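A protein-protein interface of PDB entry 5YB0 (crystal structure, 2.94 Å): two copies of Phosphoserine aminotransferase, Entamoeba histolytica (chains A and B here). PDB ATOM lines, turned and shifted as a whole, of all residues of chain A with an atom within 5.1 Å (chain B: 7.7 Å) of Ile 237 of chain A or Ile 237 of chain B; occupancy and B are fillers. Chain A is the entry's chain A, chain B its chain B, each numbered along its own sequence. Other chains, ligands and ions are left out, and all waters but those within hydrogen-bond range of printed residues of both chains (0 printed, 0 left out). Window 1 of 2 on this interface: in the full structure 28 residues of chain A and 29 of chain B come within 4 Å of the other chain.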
ATOM      1  N   THR A  24     -28.898   4.369  -5.528  1.00  0.00           N
ATOM      2  CA  THR A  24     -28.240   4.822  -4.304  1.00  0.00           C
ATOM      3  C   THR A  24     -27.554   6.227  -4.462  1.00  0.00           C
ATOM      4  O   THR A  24     -26.432   6.469  -3.996  1.00  0.00           O
ATOM      5  CB  THR A  24     -27.235   3.753  -3.851  1.00  0.00           C
ATOM      6  OG1 THR A  24     -27.808   2.438  -3.999  1.00  0.00           O
ATOM      7  CG2 THR A  24     -26.863   3.950  -2.426  1.00  0.00           C
ATOM      8  N   ILE A  37     -30.232   9.484   2.925  1.00  0.00           N
ATOM      9  CA  ILE A  37     -30.805   8.265   3.465  1.00  0.00           C
ATOM     10  C   ILE A  37     -30.043   7.869   4.717  1.00  0.00           C
ATOM     11  O   ILE A  37     -30.604   7.267   5.602  1.00  0.00           O
ATOM     12  CB  ILE A  37     -30.787   7.094   2.472  1.00  0.00           C
ATOM     13  CG1 ILE A  37     -31.483   5.881   3.097  1.00  0.00           C
ATOM     14  CG2 ILE A  37     -29.360   6.715   2.045  1.00  0.00           C
ATOM     15  CD1 ILE A  37     -32.256   5.065   2.078  1.00  0.00           C
ATOM     16  N   LEU A  38     -28.760   8.216   4.779  1.00  0.00           N
ATOM     17  CA  LEU A  38     -27.903   7.908   5.922  1.00  0.00           C
ATOM     18  C   LEU A  38     -28.186   8.862   7.089  1.00  0.00           C
ATOM     19  O   LEU A  38     -27.623   8.703   8.160  1.00  0.00           O
ATOM     20  CB  LEU A  38     -26.432   8.054   5.551  1.00  0.00           C
ATOM     21  CG  LEU A  38     -25.885   7.535   4.230  1.00  0.00           C
ATOM     22  CD1 LEU A  38     -24.567   8.238   3.963  1.00  0.00           C
ATOM     23  CD2 LEU A  38     -25.734   6.017   4.202  1.00  0.00           C
ATOM     24  N   ALA A 196     -22.846  -5.330   0.953  1.00  0.00           N
ATOM     25  CA  ALA A 196     -22.531  -5.938   2.246  1.00  0.00           C
ATOM     26  C   ALA A 196     -23.208  -5.148   3.368  1.00  0.00           C
ATOM     27  O   ALA A 196     -23.778  -4.082   3.129  1.00  0.00           O
ATOM     28  CB  ALA A 196     -21.025  -5.974   2.449  1.00  0.00           C
ATOM     29  N   PRO A 235     -29.349  -1.870   9.469  1.00  0.00           N
ATOM     30  CA  PRO A 235     -28.416  -1.272   8.486  1.00  0.00           C
ATOM     31  C   PRO A 235     -29.158  -0.606   7.318  1.00  0.00           C
ATOM     32  O   PRO A 235     -29.205  -1.156   6.194  1.00  0.00           O
ATOM     33  CB  PRO A 235     -27.638  -2.488   7.976  1.00  0.00           C
ATOM     34  CG  PRO A 235     -28.616  -3.614   8.081  1.00  0.00           C
ATOM     35  CD  PRO A 235     -29.516  -3.323   9.249  1.00  0.00           C
ATOM     36  N   VAL A 236     -29.766   0.548   7.595  1.00  0.00           N
ATOM     37  CA  VAL A 236     -30.589   1.224   6.621  1.00  0.00           C
ATOM     38  C   VAL A 236     -29.913   1.167   5.239  1.00  0.00           C
ATOM     39  O   VAL A 236     -30.448   0.554   4.328  1.00  0.00           O
ATOM     40  CB  VAL A 236     -30.773   2.696   6.969  1.00  0.00           C
ATOM     41  CG1 VAL A 236     -31.581   3.407   5.875  1.00  0.00           C
ATOM     42  CG2 VAL A 236     -31.430   2.875   8.311  1.00  0.00           C
ATOM     43  N   ILE A 237     -28.741   1.794   5.079  1.00  0.00           N
ATOM     44  CA  ILE A 237     -28.147   1.925   3.750  1.00  0.00           C
ATOM     45  C   ILE A 237     -28.080   0.594   3.029  1.00  0.00           C
ATOM     46  O   ILE A 237     -28.503   0.527   1.851  1.00  0.00           O
ATOM     47  CB  ILE A 237     -26.744   2.593   3.745  1.00  0.00           C
ATOM     48  CG1 ILE A 237     -26.192   2.692   2.329  1.00  0.00           C
ATOM     49  CG2 ILE A 237     -25.723   1.816   4.552  1.00  0.00           C
ATOM     50  CD1 ILE A 237     -27.068   3.453   1.359  1.00  0.00           C
ATOM     51  N   SER A 238     -27.584  -0.464   3.687  1.00  0.00           N
ATOM     52  CA  SER A 238     -27.477  -1.773   2.998  1.00  0.00           C
ATOM     53  C   SER A 238     -28.854  -2.296   2.573  1.00  0.00           C
ATOM     54  O   SER A 238     -29.029  -2.746   1.443  1.00  0.00           O
ATOM     55  CB  SER A 238     -26.790  -2.814   3.860  1.00  0.00           C
ATOM     56  OG  SER A 238     -25.439  -2.442   4.094  1.00  0.00           O
ATOM     57  N   ILE A 239     -29.829  -2.193   3.480  1.00  0.00           N
ATOM     58  CA  ILE A 239     -31.177  -2.610   3.200  1.00  0.00           C
ATOM     59  C   ILE A 239     -31.690  -1.927   1.960  1.00  0.00           C
ATOM     60  O   ILE A 239     -32.423  -2.539   1.146  1.00  0.00           O
ATOM     61  CB  ILE A 239     -32.078  -2.273   4.365  1.00  0.00           C
ATOM     62  CG1 ILE A 239     -31.807  -3.277   5.474  1.00  0.00           C
ATOM     63  CG2 ILE A 239     -33.552  -2.331   3.955  1.00  0.00           C
ATOM     64  CD1 ILE A 239     -32.396  -2.894   6.827  1.00  0.00           C
ATOM     65  N   PHE A 240     -31.314  -0.655   1.814  1.00  0.00           N
ATOM     66  CA  PHE A 240     -31.728   0.102   0.661  1.00  0.00           C
ATOM     67  C   PHE A 240     -31.137  -0.461  -0.628  1.00  0.00           C
ATOM     68  O   PHE A 240     -31.811  -0.477  -1.647  1.00  0.00           O
ATOM     69  CB  PHE A 240     -31.368   1.561   0.812  1.00  0.00           C
ATOM     70  CG  PHE A 240     -31.930   2.421  -0.270  1.00  0.00           C
ATOM     71  CD1 PHE A 240     -33.218   2.893  -0.178  1.00  0.00           C
ATOM     72  CD2 PHE A 240     -31.155   2.758  -1.383  1.00  0.00           C
ATOM     73  CE1 PHE A 240     -33.752   3.688  -1.177  1.00  0.00           C
ATOM     74  CE2 PHE A 240     -31.668   3.570  -2.365  1.00  0.00           C
ATOM     75  CZ  PHE A 240     -32.977   4.037  -2.261  1.00  0.00           C
ATOM     76  N   THR A 241     -29.910  -0.955  -0.598  1.00  0.00           N
ATOM     77  CA  THR A 241     -29.422  -1.622  -1.787  1.00  0.00           C
ATOM     78  C   THR A 241     -30.329  -2.795  -2.118  1.00  0.00           C
ATOM     79  O   THR A 241     -30.593  -3.033  -3.294  1.00  0.00           O
ATOM     80  CB  THR A 241     -27.964  -2.105  -1.686  1.00  0.00           C
ATOM     81  OG1 THR A 241     -27.843  -3.066  -0.652  1.00  0.00           O
ATOM     82  CG2 THR A 241     -27.051  -0.983  -1.363  1.00  0.00           C
ATOM     83  N   THR B  24     -18.898  10.202   0.563  1.00  0.00           N
ATOM     84  CA  THR B  24     -19.544   8.970   0.135  1.00  0.00           C
ATOM     85  C   THR B  24     -20.131   9.116  -1.289  1.00  0.00           C
ATOM     86  O   THR B  24     -21.298   8.820  -1.538  1.00  0.00           O
ATOM     87  CB  THR B  24     -20.601   8.600   1.162  1.00  0.00           C
ATOM     88  OG1 THR B  24     -20.058   8.772   2.475  1.00  0.00           O
ATOM     89  CG2 THR B  24     -20.980   7.200   1.024  1.00  0.00           C
ATOM     90  N   ALA B  25     -19.277   9.652  -2.190  1.00  0.00           N
ATOM     91  CA  ALA B  25     -19.403   9.581  -3.644  1.00  0.00           C
ATOM     92  C   ALA B  25     -18.734   8.284  -4.080  1.00  0.00           C
ATOM     93  O   ALA B  25     -18.694   7.955  -5.250  1.00  0.00           O
ATOM     94  CB  ALA B  25     -18.702  10.777  -4.281  1.00  0.00           C
ATOM     95  N   LYS B  26     -18.186   7.554  -3.120  1.00  0.00           N
ATOM     96  CA  LYS B  26     -17.532   6.285  -3.394  1.00  0.00           C
ATOM     97  C   LYS B  26     -18.521   5.209  -3.812  1.00  0.00           C
ATOM     98  O   LYS B  26     -18.164   4.237  -4.483  1.00  0.00           O
ATOM     99  CB  LYS B  26     -16.708   5.872  -2.173  1.00  0.00           C
ATOM    100  CG  LYS B  26     -15.341   6.568  -2.118  1.00  0.00           C
ATOM    101  CD  LYS B  26     -15.396   8.099  -2.203  1.00  0.00           C
ATOM    102  CE  LYS B  26     -14.006   8.718  -2.217  1.00  0.00           C
ATOM    103  NZ  LYS B  26     -13.766   9.542  -0.997  1.00  0.00           N
ATOM    104  N   ALA B  27     -19.779   5.416  -3.440  1.00  0.00           N
ATOM    105  CA  ALA B  27     -20.853   4.582  -3.948  1.00  0.00           C
ATOM    106  C   ALA B  27     -20.809   4.624  -5.482  1.00  0.00           C
ATOM    107  O   ALA B  27     -21.015   3.605  -6.136  1.00  0.00           O
ATOM    108  CB  ALA B  27     -22.196   5.059  -3.418  1.00  0.00           C
ATOM    109  N   SER B  36     -17.516   0.696  -7.540  1.00  0.00           N
ATOM    110  CA  SER B  36     -18.169   1.292  -6.364  1.00  0.00           C
ATOM    111  C   SER B  36     -17.546   0.766  -5.093  1.00  0.00           C
ATOM    112  O   SER B  36     -17.017  -0.319  -5.068  1.00  0.00           O
ATOM    113  CB  SER B  36     -19.690   0.970  -6.343  1.00  0.00           C
ATOM    114  OG  SER B  36     -20.244   1.063  -5.035  1.00  0.00           O
ATOM    115  N   ILE B  37     -17.646   1.520  -4.020  1.00  0.00           N
ATOM    116  CA  ILE B  37     -17.220   0.974  -2.761  1.00  0.00           C
ATOM    117  C   ILE B  37     -18.058  -0.253  -2.425  1.00  0.00           C
ATOM    118  O   ILE B  37     -17.555  -1.198  -1.817  1.00  0.00           O
ATOM    119  CB  ILE B  37     -17.264   2.000  -1.619  1.00  0.00           C
ATOM    120  CG1 ILE B  37     -16.659   1.390  -0.367  1.00  0.00           C
ATOM    121  CG2 ILE B  37     -18.667   2.526  -1.361  1.00  0.00           C
ATOM    122  CD1 ILE B  37     -15.862   2.388   0.437  1.00  0.00           C
ATOM    123  N   LEU B  38     -19.325  -0.253  -2.836  1.00  0.00           N
ATOM    124  CA  LEU B  38     -20.242  -1.358  -2.505  1.00  0.00           C
ATOM    125  C   LEU B  38     -19.948  -2.627  -3.352  1.00  0.00           C
ATOM    126  O   LEU B  38     -20.544  -3.669  -3.139  1.00  0.00           O
ATOM    127  CB  LEU B  38     -21.696  -0.934  -2.746  1.00  0.00           C
ATOM    128  CG  LEU B  38     -22.195   0.430  -2.306  1.00  0.00           C
ATOM    129  CD1 LEU B  38     -23.504   0.739  -3.005  1.00  0.00           C
ATOM    130  CD2 LEU B  38     -22.329   0.510  -0.806  1.00  0.00           C
ATOM    131  N   TRP B  47      -9.453  -2.095   0.238  1.00  0.00           N
ATOM    132  CA  TRP B  47     -10.251  -2.040   1.446  1.00  0.00           C
ATOM    133  C   TRP B  47      -9.394  -2.191   2.710  1.00  0.00           C
ATOM    134  O   TRP B  47      -9.576  -1.463   3.686  1.00  0.00           O
ATOM    135  CB  TRP B  47     -11.379  -3.087   1.458  1.00  0.00           C
ATOM    136  CG  TRP B  47     -12.184  -2.897   2.702  1.00  0.00           C
ATOM    137  CD1 TRP B  47     -12.301  -3.769   3.737  1.00  0.00           C
ATOM    138  CD2 TRP B  47     -12.889  -1.707   3.094  1.00  0.00           C
ATOM    139  NE1 TRP B  47     -13.043  -3.207   4.730  1.00  0.00           N
ATOM    140  CE2 TRP B  47     -13.419  -1.944   4.361  1.00  0.00           C
ATOM    141  CE3 TRP B  47     -13.126  -0.467   2.480  1.00  0.00           C
ATOM    142  CZ2 TRP B  47     -14.185  -1.012   5.039  1.00  0.00           C
ATOM    143  CZ3 TRP B  47     -13.887   0.483   3.164  1.00  0.00           C
ATOM    144  CH2 TRP B  47     -14.418   0.193   4.431  1.00  0.00           C
ATOM    145  N   ALA B 195     -22.740   6.495   9.752  1.00  0.00           N
ATOM    146  CA  ALA B 195     -24.069   5.998   9.375  1.00  0.00           C
ATOM    147  C   ALA B 195     -24.403   4.773  10.172  1.00  0.00           C
ATOM    148  O   ALA B 195     -23.525   4.148  10.722  1.00  0.00           O
ATOM    149  CB  ALA B 195     -24.101   5.688   7.898  1.00  0.00           C
ATOM    150  N   ALA B 196     -25.678   4.416  10.232  1.00  0.00           N
ATOM    151  CA  ALA B 196     -26.108   3.142  10.847  1.00  0.00           C
ATOM    152  C   ALA B 196     -25.490   1.978  10.099  1.00  0.00           C
ATOM    153  O   ALA B 196     -24.999   2.131   8.965  1.00  0.00           O
ATOM    154  CB  ALA B 196     -27.627   3.014  10.809  1.00  0.00           C
ATOM    155  N   GLY B 197     -25.511   0.814  10.728  1.00  0.00           N
ATOM    156  CA  GLY B 197     -24.977  -0.380  10.106  1.00  0.00           C
ATOM    157  C   GLY B 197     -23.535  -0.706  10.439  1.00  0.00           C
ATOM    158  O   GLY B 197     -22.978  -1.668   9.878  1.00  0.00           O
ATOM    159  N   VAL B 198     -22.909   0.055  11.337  1.00  0.00           N
ATOM    160  CA  VAL B 198     -21.691  -0.425  11.967  1.00  0.00           C
ATOM    161  C   VAL B 198     -21.665  -0.011  13.405  1.00  0.00           C
ATOM    162  O   VAL B 198     -22.185   1.057  13.770  1.00  0.00           O
ATOM    163  CB  VAL B 198     -20.451   0.112  11.274  1.00  0.00           C
ATOM    164  CG1 VAL B 198     -20.355   1.624  11.429  1.00  0.00           C
ATOM    165  CG2 VAL B 198     -19.207  -0.559  11.822  1.00  0.00           C
ATOM    166  N   PRO B 234     -17.337  -7.553   6.745  1.00  0.00           N
ATOM    167  CA  PRO B 234     -17.781  -6.454   7.577  1.00  0.00           C
ATOM    168  C   PRO B 234     -18.712  -5.568   6.768  1.00  0.00           C
ATOM    169  O   PRO B 234     -18.879  -5.838   5.571  1.00  0.00           O
ATOM    170  CB  PRO B 234     -16.493  -5.735   7.891  1.00  0.00           C
ATOM    171  CG  PRO B 234     -15.664  -5.931   6.656  1.00  0.00           C
ATOM    172  CD  PRO B 234     -16.050  -7.263   6.088  1.00  0.00           C
ATOM    173  N   PRO B 235     -19.313  -4.533   7.408  1.00  0.00           N
ATOM    174  CA  PRO B 235     -20.158  -3.572   6.722  1.00  0.00           C
ATOM    175  C   PRO B 235     -19.296  -2.505   6.014  1.00  0.00           C
ATOM    176  O   PRO B 235     -19.020  -1.415   6.550  1.00  0.00           O
ATOM    177  CB  PRO B 235     -20.982  -2.986   7.839  1.00  0.00           C
ATOM    178  CG  PRO B 235     -20.093  -3.077   9.023  1.00  0.00           C
ATOM    179  CD  PRO B 235     -19.203  -4.259   8.839  1.00  0.00           C
ATOM    180  N   VAL B 236     -18.855  -2.822   4.805  1.00  0.00           N
ATOM    181  CA  VAL B 236     -17.960  -1.923   4.112  1.00  0.00           C
ATOM    182  C   VAL B 236     -18.466  -0.481   4.173  1.00  0.00           C
ATOM    183  O   VAL B 236     -17.833   0.351   4.784  1.00  0.00           O
ATOM    184  CB  VAL B 236     -17.740  -2.341   2.639  1.00  0.00           C
ATOM    185  CG1 VAL B 236     -16.880  -1.306   1.908  1.00  0.00           C
ATOM    186  CG2 VAL B 236     -17.092  -3.724   2.558  1.00  0.00           C
ATOM    187  N   ILE B 237     -19.605  -0.198   3.550  1.00  0.00           N
ATOM    188  CA  ILE B 237     -20.087   1.182   3.369  1.00  0.00           C
ATOM    189  C   ILE B 237     -20.235   1.943   4.687  1.00  0.00           C
ATOM    190  O   ILE B 237     -19.889   3.138   4.765  1.00  0.00           O
ATOM    191  CB  ILE B 237     -21.452   1.204   2.659  1.00  0.00           C
ATOM    192  CG1 ILE B 237     -21.992   2.611   2.490  1.00  0.00           C
ATOM    193  CG2 ILE B 237     -22.506   0.449   3.466  1.00  0.00           C
ATOM    194  CD1 ILE B 237     -21.085   3.509   1.689  1.00  0.00           C
ATOM    195  N   SER B 238     -20.747   1.274   5.730  1.00  0.00           N
ATOM    196  CA  SER B 238     -20.942   1.971   7.001  1.00  0.00           C
ATOM    197  C   SER B 238     -19.588   2.346   7.549  1.00  0.00           C
ATOM    198  O   SER B 238     -19.340   3.501   7.895  1.00  0.00           O
ATOM    199  CB  SER B 238     -21.739   1.148   8.006  1.00  0.00           C
ATOM    200  OG  SER B 238     -23.130   1.097   7.657  1.00  0.00           O
ATOM    201  N   ILE B 239     -18.688   1.378   7.568  1.00  0.00           N
ATOM    202  CA  ILE B 239     -17.311   1.639   7.998  1.00  0.00           C
ATOM    203  C   ILE B 239     -16.728   2.827   7.283  1.00  0.00           C
ATOM    204  O   ILE B 239     -16.048   3.653   7.907  1.00  0.00           O
ATOM    205  CB  ILE B 239     -16.401   0.438   7.754  1.00  0.00           C
ATOM    206  CG1 ILE B 239     -16.725  -0.634   8.780  1.00  0.00           C
ATOM    207  CG2 ILE B 239     -14.945   0.838   7.869  1.00  0.00           C
ATOM    208  CD1 ILE B 239     -16.146  -1.985   8.440  1.00  0.00           C
ATOM    209  N   PHE B 240     -16.983   2.936   5.984  1.00  0.00           N
ATOM    210  CA  PHE B 240     -16.472   4.084   5.255  1.00  0.00           C
ATOM    211  C   PHE B 240     -16.919   5.383   5.892  1.00  0.00           C
ATOM    212  O   PHE B 240     -16.108   6.231   6.164  1.00  0.00           O
ATOM    213  CB  PHE B 240     -16.891   4.060   3.815  1.00  0.00           C
ATOM    214  CG  PHE B 240     -16.188   5.083   2.998  1.00  0.00           C
ATOM    215  CD1 PHE B 240     -14.883   4.854   2.553  1.00  0.00           C
ATOM    216  CD2 PHE B 240     -16.789   6.281   2.699  1.00  0.00           C
ATOM    217  CE1 PHE B 240     -14.224   5.780   1.798  1.00  0.00           C
ATOM    218  CE2 PHE B 240     -16.121   7.213   1.935  1.00  0.00           C
ATOM    219  CZ  PHE B 240     -14.843   6.958   1.498  1.00  0.00           C
ATOM    220  N   THR B 241     -18.206   5.504   6.197  1.00  0.00           N
ATOM    221  CA  THR B 241     -18.732   6.721   6.821  1.00  0.00           C
ATOM    222  C   THR B 241     -17.975   7.022   8.082  1.00  0.00           C
ATOM    223  O   THR B 241     -17.767   8.189   8.398  1.00  0.00           O
ATOM    224  CB  THR B 241     -20.206   6.611   7.223  1.00  0.00           C
ATOM    225  OG1 THR B 241     -20.367   5.537   8.142  1.00  0.00           O
ATOM    226  CG2 THR B 241     -21.086   6.323   6.045  1.00  0.00           C
ATOM    227  N   VAL B 242     -17.572   5.993   8.822  1.00  0.00           N
ATOM    228  CA  VAL B 242     -16.764   6.232  10.026  1.00  0.00           C
ATOM    229  C   VAL B 242     -15.390   6.827   9.680  1.00  0.00           C
ATOM    230  O   VAL B 242     -14.934   7.787  10.314  1.00  0.00           O
ATOM    231  CB  VAL B 242     -16.586   4.953  10.856  1.00  0.00           C
ATOM    232  CG1 VAL B 242     -15.555   5.164  11.954  1.00  0.00           C
ATOM    233  CG2 VAL B 242     -17.915   4.543  11.471  1.00  0.00           C
ATOM    234  N   ASN B 243     -14.741   6.241   8.671  1.00  0.00           N
ATOM    235  CA  ASN B 243     -13.476   6.757   8.146  1.00  0.00           C
ATOM    236  C   ASN B 243     -13.558   8.234   7.800  1.00  0.00           C
ATOM    237  O   ASN B 243     -12.624   8.979   8.076  1.00  0.00           O
ATOM    238  CB  ASN B 243     -13.114   6.005   6.872  1.00  0.00           C
ATOM    239  CG  ASN B 243     -11.809   6.462   6.282  1.00  0.00           C
ATOM    240  OD1 ASN B 243     -11.758   7.495   5.623  1.00  0.00           O
ATOM    241  ND2 ASN B 243     -10.755   5.659   6.470  1.00  0.00           N
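The backbone carbonyl oxygen of Ala 196 of chain A is in hydrogen-bond range of the side-chain hydroxyl of Ser 238 of chain A, at 2.5 Å.
Ala 196 of chain A touches Pro 234 of chain B. Gly 197 of chain B touches Pro 235 of chain A (CA to CA, 3.9 Å). CG2 of Ile 237 of chain A touches CG2 of Ile 237 of chain B (3.7 Å).
Of chain B, only Ile 237 (3.7 Å) comes within 4 Å of Ile 237 of chain A. Of chain A, only Ile 237 comes within 4 Å of Ile 237 of chain B. Of the printed residues of chain A, Gly 197 of chain B touches Pro 235. Of the printed residues of chain B, Pro 235 of chain A touches Gly 197 (3.9 Å). The nearest residue of chain A that does not touch Ile 237 of chain B is Ser 238 of chain A (4.2 Å). The nearest printed residue of chain B that does not touch Ala 196 of chain A is Val 236 of chain B (4.5 Å).
Along chain B the printed residues that touch a printed residue of chain A span positions 197 to 237. Of the 11 printed residues of chain A, 3 touch a printed residue of chain B. Hydrophobic or aromatic side chains of chain A that line the printed part of chain B: Ala 196 and Ile 237. Among the printed residues, 3 pairs touch across the chains. Among the printed residues, no Asp or Glu carboxylate lies within 4 Å of a Lys or Arg side-chain nitrogen of the other chain.
Ile 237 of chain A touches its own counterpart, Ile 237 of chain B. 11 positions are printed for both chains.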
